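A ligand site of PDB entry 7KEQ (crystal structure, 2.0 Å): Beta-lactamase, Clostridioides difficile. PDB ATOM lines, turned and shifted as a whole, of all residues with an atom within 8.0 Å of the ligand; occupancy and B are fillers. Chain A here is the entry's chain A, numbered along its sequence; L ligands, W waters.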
ATOM      1  N   ILE A 239      -7.228  19.994  18.521  1.00  0.00           N
ATOM      2  CA  ILE A 239      -6.956  20.840  17.372  1.00  0.00           C
ATOM      3  C   ILE A 239      -7.010  22.313  17.790  1.00  0.00           C
ATOM      4  O   ILE A 239      -7.559  22.694  18.822  1.00  0.00           O
ATOM      5  CB  ILE A 239      -7.923  20.584  16.201  1.00  0.00           C
ATOM      6  CG1 ILE A 239      -9.329  21.015  16.560  1.00  0.00           C
ATOM      7  CG2 ILE A 239      -7.912  19.109  15.778  1.00  0.00           C
ATOM      8  CD1 ILE A 239     -10.182  21.254  15.359  1.00  0.00           C
ATOM      9  N   ASP A 240      -6.410  23.149  16.940  1.00  0.00           N
ATOM     10  CA  ASP A 240      -6.305  24.579  17.182  1.00  0.00           C
ATOM     11  C   ASP A 240      -7.335  25.281  16.303  1.00  0.00           C
ATOM     12  O   ASP A 240      -7.210  25.263  15.082  1.00  0.00           O
ATOM     13  CB  ASP A 240      -4.892  25.065  16.840  1.00  0.00           C
ATOM     14  CG  ASP A 240      -4.668  26.515  17.214  1.00  0.00           C
ATOM     15  OD1 ASP A 240      -5.631  27.234  17.561  1.00  0.00           O
ATOM     16  OD2 ASP A 240      -3.496  26.957  17.116  1.00  0.00           O
ATOM     17  N   VAL A 241      -8.324  25.910  16.921  1.00  0.00           N
ATOM     18  CA  VAL A 241      -9.366  26.589  16.156  1.00  0.00           C
ATOM     19  C   VAL A 241      -9.238  28.109  16.279  1.00  0.00           C
ATOM     20  O   VAL A 241     -10.175  28.828  15.942  1.00  0.00           O
ATOM     21  CB  VAL A 241     -10.765  26.105  16.558  1.00  0.00           C
ATOM     22  CG1 VAL A 241     -11.009  24.682  16.038  1.00  0.00           C
ATOM     23  CG2 VAL A 241     -10.956  26.185  18.067  1.00  0.00           C
ATOM     24  N   ASN A 242      -8.092  28.608  16.746  1.00  0.00           N
ATOM     25  CA  ASN A 242      -7.887  30.037  17.046  1.00  0.00           C
ATOM     26  C   ASN A 242      -9.022  30.616  17.883  1.00  0.00           C
ATOM     27  O   ASN A 242      -9.551  31.694  17.610  1.00  0.00           O
ATOM     28  CB  ASN A 242      -7.672  30.870  15.778  1.00  0.00           C
ATOM     29  CG  ASN A 242      -6.499  30.383  14.940  1.00  0.00           C
ATOM     30  OD1 ASN A 242      -5.374  30.219  15.438  1.00  0.00           O
ATOM     31  ND2 ASN A 242      -6.749  30.162  13.662  1.00  0.00           N
ATOM     32  N   ASP A 243      -9.407  29.880  18.921  1.00  0.00           N
ATOM     33  CA  ASP A 243     -10.324  30.376  19.936  1.00  0.00           C
ATOM     34  C   ASP A 243      -9.937  29.690  21.236  1.00  0.00           C
ATOM     35  O   ASP A 243     -10.265  28.517  21.438  1.00  0.00           O
ATOM     36  CB  ASP A 243     -11.783  30.095  19.562  1.00  0.00           C
ATOM     37  CG  ASP A 243     -12.768  30.824  20.455  1.00  0.00           C
ATOM     38  OD1 ASP A 243     -12.374  31.305  21.550  1.00  0.00           O
ATOM     39  OD2 ASP A 243     -13.945  30.913  20.062  1.00  0.00           O
ATOM     40  N   VAL A 248     -11.381  22.082  21.247  1.00  0.00           N
ATOM     41  CA  VAL A 248     -11.946  21.171  20.268  1.00  0.00           C
ATOM     42  C   VAL A 248     -10.994  20.008  20.078  1.00  0.00           C
ATOM     43  O   VAL A 248      -9.763  20.193  20.081  1.00  0.00           O
ATOM     44  CB  VAL A 248     -12.245  21.896  18.940  1.00  0.00           C
ATOM     45  CG1 VAL A 248     -12.932  20.946  17.932  1.00  0.00           C
ATOM     46  CG2 VAL A 248     -13.116  23.113  19.201  1.00  0.00           C
ATOM     47  N   PHE A 267     -16.109  14.403  10.350  1.00  0.00           N
ATOM     48  CA  PHE A 267     -15.326  14.977  11.438  1.00  0.00           C
ATOM     49  C   PHE A 267     -16.055  14.661  12.725  1.00  0.00           C
ATOM     50  O   PHE A 267     -17.210  15.059  12.908  1.00  0.00           O
ATOM     51  CB  PHE A 267     -15.121  16.484  11.277  1.00  0.00           C
ATOM     52  CG  PHE A 267     -14.160  17.055  12.310  1.00  0.00           C
ATOM     53  CD1 PHE A 267     -12.838  16.643  12.338  1.00  0.00           C
ATOM     54  CD2 PHE A 267     -14.588  17.986  13.227  1.00  0.00           C
ATOM     55  CE1 PHE A 267     -11.957  17.169  13.277  1.00  0.00           C
ATOM     56  CE2 PHE A 267     -13.707  18.504  14.171  1.00  0.00           C
ATOM     57  CZ  PHE A 267     -12.399  18.099  14.193  1.00  0.00           C
ATOM     58  N   PRO A 294     -11.317  16.783   5.669  1.00  0.00           N
ATOM     59  CA  PRO A 294     -10.881  18.159   5.969  1.00  0.00           C
ATOM     60  C   PRO A 294     -11.926  19.230   5.665  1.00  0.00           C
ATOM     61  O   PRO A 294     -12.037  20.222   6.408  1.00  0.00           O
ATOM     62  CB  PRO A 294      -9.625  18.326   5.106  1.00  0.00           C
ATOM     63  CG  PRO A 294      -9.072  16.929   5.018  1.00  0.00           C
ATOM     64  CD  PRO A 294     -10.269  16.006   4.984  1.00  0.00           C
ATOM     65  N   LYS A 297     -14.530  19.095   8.371  1.00  0.00           N
ATOM     66  CA  LYS A 297     -13.978  19.664   9.595  1.00  0.00           C
ATOM     67  C   LYS A 297     -14.097  21.189   9.584  1.00  0.00           C
ATOM     68  O   LYS A 297     -14.352  21.813  10.619  1.00  0.00           O
ATOM     69  CB  LYS A 297     -12.521  19.248   9.755  1.00  0.00           C
ATOM     70  CG  LYS A 297     -11.713  20.082  10.752  1.00  0.00           C
ATOM     71  CD  LYS A 297     -10.323  19.470  10.897  1.00  0.00           C
ATOM     72  CE  LYS A 297      -9.380  20.331  11.713  1.00  0.00           C
ATOM     73  NZ  LYS A 297      -8.012  19.711  11.692  1.00  0.00           N
ATOM     74  N   GLU A 298     -13.895  21.796   8.406  1.00  0.00           N
ATOM     75  CA  GLU A 298     -14.111  23.240   8.279  1.00  0.00           C
ATOM     76  C   GLU A 298     -15.562  23.607   8.571  1.00  0.00           C
ATOM     77  O   GLU A 298     -15.834  24.561   9.305  1.00  0.00           O
ATOM     78  CB  GLU A 298     -13.695  23.688   6.871  1.00  0.00           C
ATOM     79  CG  GLU A 298     -13.754  25.174   6.608  1.00  0.00           C
ATOM     80  CD  GLU A 298     -13.820  25.483   5.112  1.00  0.00           C
ATOM     81  OE1 GLU A 298     -14.813  26.115   4.670  1.00  0.00           O
ATOM     82  OE2 GLU A 298     -12.893  25.100   4.374  1.00  0.00           O
ATOM     83  N   ILE A 301     -16.206  23.359  12.231  1.00  0.00           N
ATOM     84  CA  ILE A 301     -15.642  24.454  13.012  1.00  0.00           C
ATOM     85  C   ILE A 301     -16.517  25.688  12.884  1.00  0.00           C
ATOM     86  O   ILE A 301     -16.693  26.455  13.849  1.00  0.00           O
ATOM     87  CB  ILE A 301     -14.190  24.727  12.557  1.00  0.00           C
ATOM     88  CG1 ILE A 301     -13.283  23.611  13.087  1.00  0.00           C
ATOM     89  CG2 ILE A 301     -13.715  26.056  13.086  1.00  0.00           C
ATOM     90  CD1 ILE A 301     -11.844  23.716  12.625  1.00  0.00           C
ATOM     91  N   ASN A 302     -17.107  25.897  11.699  1.00  0.00           N
ATOM     92  CA  ASN A 302     -18.025  27.010  11.506  1.00  0.00           C
ATOM     93  C   ASN A 302     -19.279  26.844  12.352  1.00  0.00           C
ATOM     94  O   ASN A 302     -19.783  27.806  12.936  1.00  0.00           O
ATOM     95  CB  ASN A 302     -18.412  27.119  10.035  1.00  0.00           C
ATOM     96  CG  ASN A 302     -17.301  27.697   9.204  1.00  0.00           C
ATOM     97  OD1 ASN A 302     -16.414  28.383   9.717  1.00  0.00           O
ATOM     98  ND2 ASN A 302     -17.333  27.433   7.903  1.00  0.00           N
ATOM     99  N   LYS A 305     -18.296  27.623  15.979  1.00  0.00           N
ATOM    100  CA  LYS A 305     -18.094  29.032  16.249  1.00  0.00           C
ATOM    101  C   LYS A 305     -19.412  29.802  16.209  1.00  0.00           C
ATOM    102  O   LYS A 305     -19.579  30.774  16.955  1.00  0.00           O
ATOM    103  CB  LYS A 305     -17.088  29.616  15.272  1.00  0.00           C
ATOM    104  CG  LYS A 305     -15.652  29.240  15.648  1.00  0.00           C
ATOM    105  CD  LYS A 305     -14.631  29.749  14.645  1.00  0.00           C
ATOM    106  CE  LYS A 305     -13.230  29.419  15.113  1.00  0.00           C
ATOM    107  NZ  LYS A 305     -12.249  29.563  13.995  1.00  0.00           N
HETATM  108  C1  LIG L   1      -8.213  24.356  11.624  1.00  0.00           C
HETATM  109  C2  LIG L   1      -7.673  27.523   9.976  1.00  0.00           C
HETATM  110  C3  LIG L   1      -8.493  26.212   9.939  1.00  0.00           C
HETATM  111  C4  LIG L   1      -8.905  25.648  11.311  1.00  0.00           C
HETATM  112  C5  LIG L   1      -7.340  27.187  12.352  1.00  0.00           C
HETATM  113  C6  LIG L   1      -7.600  28.288  11.308  1.00  0.00           C
HETATM  114  C7  LIG L   1      -9.593  27.744  12.295  1.00  0.00           C
HETATM  115  N1  LIG L   1      -8.700  26.813  12.136  1.00  0.00           N
HETATM  116  N2  LIG L   1      -8.988  28.687  11.598  1.00  0.00           N
HETATM  117  N3  LIG L   1      -8.070  23.483  10.619  1.00  0.00           N
HETATM  118  O1  LIG L   1     -10.654  27.735  12.888  1.00  0.00           O
HETATM  119  O2  LIG L   1      -9.563  29.716  11.130  1.00  0.00           O
HETATM  120  O3  LIG L   1     -10.182  31.050  13.129  1.00  0.00           O
HETATM  121  O4  LIG L   1      -8.278  31.751  11.803  1.00  0.00           O
HETATM  122  O5  LIG L   1     -10.519  31.985  10.941  1.00  0.00           O
HETATM  123  O6  LIG L   1      -7.821  24.102  12.748  1.00  0.00           O
HETATM  124  S1  LIG L   1      -9.625  31.135  11.766  1.00  0.00           S
HETATM  125  O   HOH W   1     -12.101  32.230  15.799  1.00  0.00           O
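The side-chain amino group (NZ) of Lys 305 lies within salt-bridge range of an oxygen (O3) of the ligand, at 2.7 Å. The backbone carbonyl oxygen (O) of Asp 240 sits close to an oxygen (O6) of the ligand (2.7 Å). The side-chain amide nitrogen of Asn 242 is in hydrogen-bond range of an oxygen (O4) of the ligand (2.9 Å).
O of Val 241 sits at hydrogen-bond distance from NZ of Lys 305 (2.9 Å). The side-chain carboxylate of Asp 240 lies within hydrogen-bond range of the backbone NH of Asn 242 (2.9 Å).
An oxygen (O1) of the ligand lies close to the backbone carbonyl oxygen (O) of Val 241, 3.3 Å away. CE of Lys 297 touches N3 of the ligand (3.6 Å). Ile 301 touches the ligand (CG2 to O1, 3.5 Å). Hydrophobic or aromatic side chains within 4 Å of the ligand: Ile 301.
Water W1 lies within hydrogen-bond range of the backbone carbonyl oxygen (O) of Asn 242, the side-chain amino group (NZ) of Lys 305 and an oxygen (O3) of the ligand.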
